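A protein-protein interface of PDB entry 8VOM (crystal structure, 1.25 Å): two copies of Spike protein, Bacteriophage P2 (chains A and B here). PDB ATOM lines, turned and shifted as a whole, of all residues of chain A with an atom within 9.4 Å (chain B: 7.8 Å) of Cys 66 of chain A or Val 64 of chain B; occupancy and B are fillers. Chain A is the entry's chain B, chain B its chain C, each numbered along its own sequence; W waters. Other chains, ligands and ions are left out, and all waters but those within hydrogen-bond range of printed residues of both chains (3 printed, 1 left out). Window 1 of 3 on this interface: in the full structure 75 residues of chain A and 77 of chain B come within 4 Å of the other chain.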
ATOM      1  N   VAL A  49      -8.501   3.607  14.400  1.00  0.00           N
ATOM      2  CA  VAL A  49      -8.028   2.247  14.190  1.00  0.00           C
ATOM      3  C   VAL A  49      -8.616   1.766  12.878  1.00  0.00           C
ATOM      4  O   VAL A  49      -9.833   1.809  12.685  1.00  0.00           O
ATOM      5  CB  VAL A  49      -8.421   1.310  15.343  1.00  0.00           C
ATOM      6  CG1 VAL A  49      -8.032  -0.120  15.006  1.00  0.00           C
ATOM      7  CG2 VAL A  49      -7.775   1.792  16.628  1.00  0.00           C
ATOM      8  N   VAL A  51      -8.544  -1.486  10.222  1.00  0.00           N
ATOM      9  CA  VAL A  51      -8.198  -2.866   9.932  1.00  0.00           C
ATOM     10  C   VAL A  51      -8.667  -3.180   8.523  1.00  0.00           C
ATOM     11  O   VAL A  51      -9.867  -3.127   8.242  1.00  0.00           O
ATOM     12  CB  VAL A  51      -8.807  -3.822  10.960  1.00  0.00           C
ATOM     13  CG1 VAL A  51      -8.405  -5.242  10.642  1.00  0.00           C
ATOM     14  CG2 VAL A  51      -8.359  -3.466  12.358  1.00  0.00           C
ATOM     15  N   VAL A  57     -12.101 -10.624   9.906  1.00  0.00           N
ATOM     16  CA  VAL A  57     -11.714 -10.251  11.261  1.00  0.00           C
ATOM     17  C   VAL A  57     -12.564 -11.090  12.199  1.00  0.00           C
ATOM     18  O   VAL A  57     -13.795 -10.991  12.164  1.00  0.00           O
ATOM     19  CB  VAL A  57     -11.967  -8.764  11.552  1.00  0.00           C
ATOM     20  CG1 VAL A  57     -11.669  -8.452  13.026  1.00  0.00           C
ATOM     21  CG2 VAL A  57     -11.160  -7.914  10.610  1.00  0.00           C
ATOM     22  N   LEU A  59     -13.355 -11.884  16.183  1.00  0.00           N
ATOM     23  CA  LEU A  59     -13.286 -11.499  17.592  1.00  0.00           C
ATOM     24  C   LEU A  59     -13.832 -12.711  18.346  1.00  0.00           C
ATOM     25  O   LEU A  59     -15.043 -12.889  18.488  1.00  0.00           O
ATOM     26  CB  LEU A  59     -14.094 -10.241  17.810  1.00  0.00           C
ATOM     27  CG  LEU A  59     -13.704  -9.067  16.899  1.00  0.00           C
ATOM     28  CD1 LEU A  59     -14.558  -7.852  17.235  1.00  0.00           C
ATOM     29  CD2 LEU A  59     -12.252  -8.741  16.992  1.00  0.00           C
ATOM     30  N   GLU A  63     -17.459 -11.863  24.805  1.00  0.00           N
ATOM     31  CA  GLU A  63     -18.188 -10.614  24.680  1.00  0.00           C
ATOM     32  C   GLU A  63     -17.363  -9.593  23.923  1.00  0.00           C
ATOM     33  O   GLU A  63     -16.231  -9.288  24.311  1.00  0.00           O
ATOM     34  CB  GLU A  63     -18.460 -10.083  26.079  1.00  0.00           C
ATOM     35  CG  GLU A  63     -19.524  -9.063  26.232  1.00  0.00           C
ATOM     36  CD  GLU A  63     -19.819  -8.879  27.706  1.00  0.00           C
ATOM     37  OE1 GLU A  63     -20.754  -9.535  28.207  1.00  0.00           O
ATOM     38  OE2 GLU A  63     -19.070  -8.140  28.376  1.00  0.00           O
ATOM     39  N   VAL A  64     -17.957  -9.046  22.864  1.00  0.00           N
ATOM     40  CA  VAL A  64     -17.475  -7.837  22.214  1.00  0.00           C
ATOM     41  C   VAL A  64     -18.385  -6.704  22.661  1.00  0.00           C
ATOM     42  O   VAL A  64     -19.615  -6.808  22.548  1.00  0.00           O
ATOM     43  CB  VAL A  64     -17.517  -7.974  20.685  1.00  0.00           C
ATOM     44  CG1 VAL A  64     -17.097  -6.672  20.026  1.00  0.00           C
ATOM     45  CG2 VAL A  64     -16.667  -9.121  20.231  1.00  0.00           C
ATOM     46  N   VAL A  65     -17.790  -5.616  23.135  1.00  0.00           N
ATOM     47  CA  VAL A  65     -18.536  -4.454  23.589  1.00  0.00           C
ATOM     48  C   VAL A  65     -18.152  -3.273  22.714  1.00  0.00           C
ATOM     49  O   VAL A  65     -16.982  -2.886  22.663  1.00  0.00           O
ATOM     50  CB  VAL A  65     -18.260  -4.129  25.065  1.00  0.00           C
ATOM     51  CG1 VAL A  65     -18.979  -2.827  25.462  1.00  0.00           C
ATOM     52  CG2 VAL A  65     -18.667  -5.294  25.944  1.00  0.00           C
ATOM     53  N   CYS A  66     -19.140  -2.694  22.052  1.00  0.00           N
ATOM     54  CA  CYS A  66     -18.995  -1.415  21.373  1.00  0.00           C
ATOM     55  C   CYS A  66     -19.677  -0.388  22.264  1.00  0.00           C
ATOM     56  O   CYS A  66     -20.869  -0.518  22.548  1.00  0.00           O
ATOM     57  CB  CYS A  66     -19.667  -1.474  20.005  1.00  0.00           C
ATOM     58  SG  CYS A  66     -19.055  -2.736  18.903  1.00  0.00           S
ATOM     59  N   THR A  67     -18.924   0.613  22.724  1.00  0.00           N
ATOM     60  CA  THR A  67     -19.448   1.450  23.799  1.00  0.00           C
ATOM     61  C   THR A  67     -20.470   2.467  23.322  1.00  0.00           C
ATOM     62  O   THR A  67     -21.183   3.029  24.156  1.00  0.00           O
ATOM     63  CB  THR A  67     -18.322   2.142  24.563  1.00  0.00           C
ATOM     64  OG1 THR A  67     -17.575   2.924  23.630  1.00  0.00           O
ATOM     65  CG2 THR A  67     -17.446   1.137  25.269  1.00  0.00           C
ATOM     66  N   ASN A  68     -20.548   2.728  22.018  1.00  0.00           N
ATOM     67  CA  ASN A  68     -21.482   3.707  21.477  1.00  0.00           C
ATOM     68  C   ASN A  68     -22.163   3.126  20.248  1.00  0.00           C
ATOM     69  O   ASN A  68     -22.965   2.198  20.383  1.00  0.00           O
ATOM     70  CB  ASN A  68     -20.780   5.044  21.256  1.00  0.00           C
ATOM     71  CG  ASN A  68     -20.284   5.644  22.560  1.00  0.00           C
ATOM     72  OD1 ASN A  68     -19.121   5.471  22.973  1.00  0.00           O
ATOM     73  ND2 ASN A  68     -21.181   6.317  23.242  1.00  0.00           N
ATOM     74  N   ARG A  69     -21.842   3.630  19.061  1.00  0.00           N
ATOM     75  CA  ARG A  69     -22.508   3.197  17.844  1.00  0.00           C
ATOM     76  C   ARG A  69     -21.748   2.080  17.142  1.00  0.00           C
ATOM     77  O   ARG A  69     -20.513   2.048  17.125  1.00  0.00           O
ATOM     78  CB  ARG A  69     -22.653   4.376  16.882  1.00  0.00           C
ATOM     79  CG  ARG A  69     -23.453   4.050  15.631  1.00  0.00           C
ATOM     80  CD  ARG A  69     -24.056   5.282  14.954  1.00  0.00           C
ATOM     81  NE  ARG A  69     -23.074   6.351  14.867  1.00  0.00           N
ATOM     82  CZ  ARG A  69     -22.809   7.216  15.837  1.00  0.00           C
ATOM     83  NH1 ARG A  69     -23.659   7.420  16.832  1.00  0.00           N
ATOM     84  NH2 ARG A  69     -21.671   7.897  15.804  1.00  0.00           N
ATOM     85  N   LEU A  70     -22.519   1.193  16.523  1.00  0.00           N
ATOM     86  CA  LEU A  70     -22.032   0.130  15.662  1.00  0.00           C
ATOM     87  C   LEU A  70     -22.805   0.236  14.354  1.00  0.00           C
ATOM     88  O   LEU A  70     -24.042   0.280  14.361  1.00  0.00           O
ATOM     89  CB  LEU A  70     -22.265  -1.224  16.323  1.00  0.00           C
ATOM     90  CG  LEU A  70     -22.053  -2.449  15.450  1.00  0.00           C
ATOM     91  CD1 LEU A  70     -20.618  -2.545  15.012  1.00  0.00           C
ATOM     92  CD2 LEU A  70     -22.438  -3.681  16.212  1.00  0.00           C
ATOM     93  N   ILE A  71     -22.069   0.313  13.246  1.00  0.00           N
ATOM     94  CA  ILE A  71     -22.615   0.391  11.897  1.00  0.00           C
ATOM     95  C   ILE A  71     -22.105  -0.820  11.134  1.00  0.00           C
ATOM     96  O   ILE A  71     -20.907  -1.120  11.174  1.00  0.00           O
ATOM     97  CB  ILE A  71     -22.154   1.675  11.182  1.00  0.00           C
ATOM     98  CG1 ILE A  71     -22.574   2.899  11.984  1.00  0.00           C
ATOM     99  CG2 ILE A  71     -22.698   1.720   9.758  1.00  0.00           C
ATOM    100  CD1 ILE A  71     -21.959   4.173  11.497  1.00  0.00           C
ATOM    101  N   THR A  72     -23.002  -1.498  10.432  1.00  0.00           N
ATOM    102  CA  THR A  72     -22.600  -2.598   9.573  1.00  0.00           C
ATOM    103  C   THR A  72     -23.387  -2.562   8.274  1.00  0.00           C
ATOM    104  O   THR A  72     -24.491  -2.027   8.208  1.00  0.00           O
ATOM    105  CB  THR A  72     -22.756  -3.958  10.281  1.00  0.00           C
ATOM    106  OG1 THR A  72     -22.129  -4.966   9.476  1.00  0.00           O
ATOM    107  CG2 THR A  72     -24.213  -4.326  10.554  1.00  0.00           C
ATOM    108  N   GLY A  73     -22.794  -3.148   7.230  1.00  0.00           N
ATOM    109  CA  GLY A  73     -23.480  -3.327   5.966  1.00  0.00           C
ATOM    110  C   GLY A  73     -24.629  -4.304   6.081  1.00  0.00           C
ATOM    111  O   GLY A  73     -25.793  -3.957   5.880  1.00  0.00           O
ATOM    112  N   VAL B  57     -13.413  -8.263  24.419  1.00  0.00           N
ATOM    113  CA  VAL B  57     -12.871  -7.257  23.512  1.00  0.00           C
ATOM    114  C   VAL B  57     -13.766  -6.031  23.642  1.00  0.00           C
ATOM    115  O   VAL B  57     -14.964  -6.109  23.351  1.00  0.00           O
ATOM    116  CB  VAL B  57     -12.853  -7.739  22.052  1.00  0.00           C
ATOM    117  CG1 VAL B  57     -12.379  -6.620  21.122  1.00  0.00           C
ATOM    118  CG2 VAL B  57     -11.986  -8.977  21.909  1.00  0.00           C
ATOM    119  N   THR B  58     -13.191  -4.900  24.052  1.00  0.00           N
ATOM    120  CA  THR B  58     -13.934  -3.647  24.134  1.00  0.00           C
ATOM    121  C   THR B  58     -13.435  -2.695  23.058  1.00  0.00           C
ATOM    122  O   THR B  58     -12.235  -2.416  22.980  1.00  0.00           O
ATOM    123  CB  THR B  58     -13.793  -2.988  25.509  1.00  0.00           C
ATOM    124  OG1 THR B  58     -14.291  -3.878  26.505  1.00  0.00           O
ATOM    125  CG2 THR B  58     -14.595  -1.700  25.590  1.00  0.00           C
ATOM    126  N   LEU B  59     -14.369  -2.195  22.259  1.00  0.00           N
ATOM    127  CA  LEU B  59     -14.126  -1.163  21.248  1.00  0.00           C
ATOM    128  C   LEU B  59     -14.781   0.097  21.820  1.00  0.00           C
ATOM    129  O   LEU B  59     -15.986   0.311  21.687  1.00  0.00           O
ATOM    130  CB  LEU B  59     -14.712  -1.588  19.913  1.00  0.00           C
ATOM    131  CG  LEU B  59     -14.240  -2.961  19.432  1.00  0.00           C
ATOM    132  CD1 LEU B  59     -14.875  -3.303  18.083  1.00  0.00           C
ATOM    133  CD2 LEU B  59     -12.736  -3.061  19.328  1.00  0.00           C
ATOM    134  N   ASP B  60     -13.976   0.878  22.531  1.00  0.00           N
ATOM    135  CA  ASP B  60     -14.449   2.060  23.243  1.00  0.00           C
ATOM    136  C   ASP B  60     -14.223   3.258  22.334  1.00  0.00           C
ATOM    137  O   ASP B  60     -13.146   3.863  22.314  1.00  0.00           O
ATOM    138  CB  ASP B  60     -13.715   2.222  24.564  1.00  0.00           C
ATOM    139  CG  ASP B  60     -14.277   3.351  25.390  1.00  0.00           C
ATOM    140  OD1 ASP B  60     -15.252   3.980  24.937  1.00  0.00           O
ATOM    141  OD2 ASP B  60     -13.733   3.647  26.469  1.00  0.00           O
ATOM    142  N   THR B  61     -15.258   3.593  21.570  1.00  0.00           N
ATOM    143  CA  THR B  61     -15.129   4.516  20.456  1.00  0.00           C
ATOM    144  C   THR B  61     -16.509   5.063  20.153  1.00  0.00           C
ATOM    145  O   THR B  61     -17.507   4.387  20.415  1.00  0.00           O
ATOM    146  CB  THR B  61     -14.540   3.769  19.242  1.00  0.00           C
ATOM    147  OG1 THR B  61     -14.345   4.665  18.151  1.00  0.00           O
ATOM    148  CG2 THR B  61     -15.434   2.653  18.751  1.00  0.00           C
ATOM    149  N   PRO B  62     -16.604   6.266  19.586  1.00  0.00           N
ATOM    150  CA  PRO B  62     -17.923   6.744  19.165  1.00  0.00           C
ATOM    151  C   PRO B  62     -18.582   5.838  18.150  1.00  0.00           C
ATOM    152  O   PRO B  62     -19.813   5.730  18.129  1.00  0.00           O
ATOM    153  CB  PRO B  62     -17.621   8.130  18.569  1.00  0.00           C
ATOM    154  CG  PRO B  62     -16.404   8.575  19.287  1.00  0.00           C
ATOM    155  CD  PRO B  62     -15.573   7.309  19.447  1.00  0.00           C
ATOM    156  N   GLU B  63     -17.793   5.173  17.308  1.00  0.00           N
ATOM    157  CA  GLU B  63     -18.346   4.415  16.199  1.00  0.00           C
ATOM    158  C   GLU B  63     -17.423   3.284  15.797  1.00  0.00           C
ATOM    159  O   GLU B  63     -16.229   3.496  15.562  1.00  0.00           O
ATOM    160  CB  GLU B  63     -18.531   5.323  14.987  1.00  0.00           C
ATOM    161  CG  GLU B  63     -19.571   4.911  14.027  1.00  0.00           C
ATOM    162  CD  GLU B  63     -19.792   6.000  12.996  1.00  0.00           C
ATOM    163  OE1 GLU B  63     -19.020   6.114  12.014  1.00  0.00           O
ATOM    164  OE2 GLU B  63     -20.715   6.806  13.225  1.00  0.00           O
ATOM    165  N   VAL B  64     -18.004   2.092  15.696  1.00  0.00           N
ATOM    166  CA  VAL B  64     -17.375   0.938  15.075  1.00  0.00           C
ATOM    167  C   VAL B  64     -18.071   0.746  13.736  1.00  0.00           C
ATOM    168  O   VAL B  64     -19.307   0.700  13.684  1.00  0.00           O
ATOM    169  CB  VAL B  64     -17.531  -0.322  15.942  1.00  0.00           C
ATOM    170  CG1 VAL B  64     -16.981  -1.532  15.198  1.00  0.00           C
ATOM    171  CG2 VAL B  64     -16.889  -0.132  17.298  1.00  0.00           C
ATOM    172  N   VAL B  65     -17.291   0.649  12.659  1.00  0.00           N
ATOM    173  CA  VAL B  65     -17.831   0.462  11.314  1.00  0.00           C
ATOM    174  C   VAL B  65     -17.337  -0.874  10.787  1.00  0.00           C
ATOM    175  O   VAL B  65     -16.126  -1.094  10.699  1.00  0.00           O
ATOM    176  CB  VAL B  65     -17.418   1.594  10.361  1.00  0.00           C
ATOM    177  CG1 VAL B  65     -17.856   1.283   8.930  1.00  0.00           C
ATOM    178  CG2 VAL B  65     -17.977   2.905  10.857  1.00  0.00           C
ATOM    179  N   CYS B  66     -18.270  -1.761  10.451  1.00  0.00           N
ATOM    180  CA  CYS B  66     -17.973  -2.988   9.726  1.00  0.00           C
ATOM    181  C   CYS B  66     -18.426  -2.753   8.292  1.00  0.00           C
ATOM    182  O   CYS B  66     -19.602  -2.472   8.061  1.00  0.00           O
ATOM    183  CB  CYS B  66     -18.720  -4.171  10.335  1.00  0.00           C
ATOM    184  SG  CYS B  66     -18.428  -4.431  12.077  1.00  0.00           S
ATOM    185  N   THR B  67     -17.498  -2.808   7.336  1.00  0.00           N
ATOM    186  CA  THR B  67     -17.820  -2.310   6.002  1.00  0.00           C
ATOM    187  C   THR B  67     -18.705  -3.251   5.201  1.00  0.00           C
ATOM    188  O   THR B  67     -19.277  -2.817   4.202  1.00  0.00           O
ATOM    189  CB  THR B  67     -16.553  -1.989   5.212  1.00  0.00           C
ATOM    190  OG1 THR B  67     -15.748  -3.169   5.121  1.00  0.00           O
ATOM    191  CG2 THR B  67     -15.782  -0.868   5.879  1.00  0.00           C
ATOM    192  N   LEU B  70     -21.423  -8.438   9.316  1.00  0.00           N
ATOM    193  CA  LEU B  70     -21.142  -8.682  10.722  1.00  0.00           C
ATOM    194  C   LEU B  70     -21.969  -9.885  11.144  1.00  0.00           C
ATOM    195  O   LEU B  70     -23.187  -9.898  10.944  1.00  0.00           O
ATOM    196  CB  LEU B  70     -21.556  -7.471  11.548  1.00  0.00           C
ATOM    197  CG  LEU B  70     -21.587  -7.610  13.060  1.00  0.00           C
ATOM    198  CD1 LEU B  70     -20.201  -7.902  13.565  1.00  0.00           C
ATOM    199  CD2 LEU B  70     -22.147  -6.339  13.656  1.00  0.00           C
ATOM    200  N   GLU B  76     -26.960  -7.800  21.682  1.00  0.00           N
ATOM    201  CA  GLU B  76     -27.611  -6.962  22.683  1.00  0.00           C
ATOM    202  C   GLU B  76     -27.442  -5.510  22.258  1.00  0.00           C
ATOM    203  O   GLU B  76     -26.318  -5.001  22.224  1.00  0.00           O
ATOM    204  CB  GLU B  76     -26.988  -7.187  24.058  1.00  0.00           C
ATOM    205  CG  GLU B  76     -27.621  -6.381  25.154  1.00  0.00           C
ATOM    206  CD  GLU B  76     -26.880  -6.476  26.481  1.00  0.00           C
ATOM    207  OE1 GLU B  76     -26.137  -7.462  26.699  1.00  0.00           O
ATOM    208  OE2 GLU B  76     -27.063  -5.563  27.313  1.00  0.00           O
ATOM    209  N   GLN B  78     -28.433  -1.761  23.356  1.00  0.00           N
ATOM    210  CA  GLN B  78     -28.829  -1.152  24.622  1.00  0.00           C
ATOM    211  C   GLN B  78     -29.702   0.088  24.489  1.00  0.00           C
ATOM    212  O   GLN B  78     -30.559   0.317  25.356  1.00  0.00           O
ATOM    213  CB  GLN B  78     -27.568  -0.803  25.418  1.00  0.00           C
ATOM    214  CG  GLN B  78     -26.661  -1.995  25.688  1.00  0.00           C
ATOM    215  CD  GLN B  78     -25.417  -1.605  26.458  1.00  0.00           C
ATOM    216  OE1 GLN B  78     -25.089  -2.209  27.488  1.00  0.00           O
ATOM    217  NE2 GLN B  78     -24.669  -0.637  25.914  1.00  0.00           N
HETATM  218  O   HOH W   1     -19.006   2.057  19.664  1.00  0.00           O
HETATM  219  O   HOH W   2     -22.198  -0.906  25.090  1.00  0.00           O
HETATM  220  O   HOH W   3     -21.163   7.958  19.044  1.00  0.00           O
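Water W2 bridges NE2 of Gln 78 of chain B (2.6 Å) and O of Cys 66 of chain A (2.9 Å). Water W3 bridges the backbone carbonyl oxygen of Pro 62 of chain B (2.8 Å) and the guanidinium group of Arg 69 of chain A (3.3 Å). Water W1 lies within hydrogen-bond range of O of Thr 61 of chain B (2.9 Å), N of Asn 68 of chain A (2.9 Å), O of Arg 69 of chain A (3.0 Å) and N of Thr 67 of chain A (3.4 Å).
The backbone carbonyl oxygen of Glu 63 of chain A sits at hydrogen-bond distance from the backbone NH of Val 57 of chain B (3.0 Å). The backbone NH of Val 65 of chain A lies within hydrogen-bond range of the backbone carbonyl oxygen of Val 57 of chain B. The backbone NH (N) of Leu 59 of chain B sits at hydrogen-bond distance from the backbone carbonyl oxygen (O) of Val 65 of chain A, 2.7 Å away. The backbone NH of Thr 67 of chain A lies within hydrogen-bond range of the backbone carbonyl oxygen of Leu 59 of chain B, 3.1 Å away. The side-chain hydroxyl of Thr 67 of chain A sits at hydrogen-bond distance from the side-chain carboxylate of Asp 60 of chain B (2.9 Å). The side-chain hydroxyl of Thr 67 of chain A lies within hydrogen-bond range of the backbone NH of Thr 61 of chain B (3.2 Å). The backbone carbonyl oxygen of Thr 61 of chain B sits close to the side-chain amide oxygen of Asn 68 of chain A (3.2 Å). The backbone NH (N) of Arg 69 of chain A is in hydrogen-bond range of the backbone carbonyl oxygen (O) of Pro 62 of chain B (3.1 Å). The guanidinium group (NE) of Arg 69 of chain A lies within salt-bridge range of the side-chain carboxylate (OE2) of Glu 63 of chain B, 2.9 Å away. N of Val 64 of chain B lies within hydrogen-bond range of O of Arg 69 of chain A. The backbone NH (N) of Ile 71 of chain A is in hydrogen-bond range of the backbone carbonyl oxygen (O) of Val 64 of chain B (2.8 Å). The backbone carbonyl oxygen (O) of Ile 71 of chain A lies within hydrogen-bond range of the backbone NH (N) of Cys 66 of chain B, at 2.8 Å. The backbone NH (N) of Gly 73 of chain A lies within hydrogen-bond range of the backbone carbonyl oxygen (O) of Cys 66 of chain B.
Val 64 of chain A touches Val 57 of chain B, but with the chains exchanged Val 57 of chain A does not touch Val 64 of chain B (9.0 Å). Val 65 of chain A touches Val 57 of chain B, but with the chains exchanged Val 57 of chain A does not touch Val 65 of chain B (8.4 Å). Cys 66 of chain A touches Leu 59 of chain B, but with the chains exchanged Leu 59 of chain A does not touch Cys 66 of chain B (7.3 Å). Thr 67 of chain A touches Leu 59 of chain B, but with the chains exchanged Leu 59 of chain A does not touch Thr 67 of chain B (11.5 Å). Of the 24 pairs that touch across the chains among the printed residues, 1 has its exchanged pair printed and touching as well.
Printed residues of chain A that touch a printed residue of chain B: Glu 63, Val 64, Val 65, Cys 66, Thr 67, Asn 68, Arg 69, Leu 70, Ile 71, Thr 72 and Gly 73. Along chain A the printed residues that touch a printed residue of chain B span positions 63 to 73. Of the 14 printed residues of chain B, 11 touch a printed residue of chain A. Among the printed residues, Asp or Glu carboxylates within 4 Å of a Lys or Arg side-chain nitrogen of the other chain: Arg 69 of chain A with Glu 63 of chain B.
Val 57 of chain A touches none of the printed residues of chain B. Cys 66 of chain A touches just these residues of chain B: Leu 59 (3.5 Å) and Val 64 (3.7 Å). Of the printed residues of chain A, Asp 60 of chain B touches Thr 67 (2.9 Å). Of the printed residues of chain A, Pro 62 of chain B touches Asn 68 and Arg 69. Printed residues of chain A within 4 Å of Val 64 of chain B: Cys 66, Arg 69, Leu 70 and Ile 71. Val 65 of chain B touches just one residue of chain A: Ile 71 (3.5 Å). Printed residues of chain A within 4 Å of Cys 66 of chain B: Ile 71 (2.8 Å), Thr 72 (3.4 Å) and Gly 73 (3.4 Å). The nearest residue of chain B that does not touch Cys 66 of chain A is Gln 78 of chain B (5.1 Å). The nearest printed residue of chain A that does not touch Val 64 of chain B is Thr 72 of chain A (5.4 Å).
O of Val 57 of chain B touches CA of Val 64 of chain A, 3.3 Å away. O of Val 65 of chain A touches CA of Thr 58 of chain B (3.5 Å). CA of Cys 66 of chain A touches O of Leu 59 of chain B, 3.5 Å away. Val 64 of chain B touches Cys 66 of chain A (CG2 to SG, 3.7 Å). CA of Leu 70 of chain A touches O of Val 64 of chain B (3.4 Å). Leu 70 of chain B touches Leu 70 of chain A (CD2 to CD2, 3.7 Å). Ile 71 of chain A touches Glu 63 of chain B. Ile 71 of chain A touches Val 65 of chain B (O to CA, 3.5 Å). Thr 72 of chain A touches Cys 66 of chain B (CA to O, 3.4 Å). Leu 70 of chain B touches Thr 72 of chain A (CB to OG1, 3.3 Å).
The side-chain hydroxyl (OG1) of Thr 67 of chain A is in hydrogen-bond range of the side-chain amide oxygen (OD1) of Asn 68 of chain A, at 3.1 Å. OG1 of Thr 61 of chain B lies close to O of Glu 63 of chain B, at 3.4 Å.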
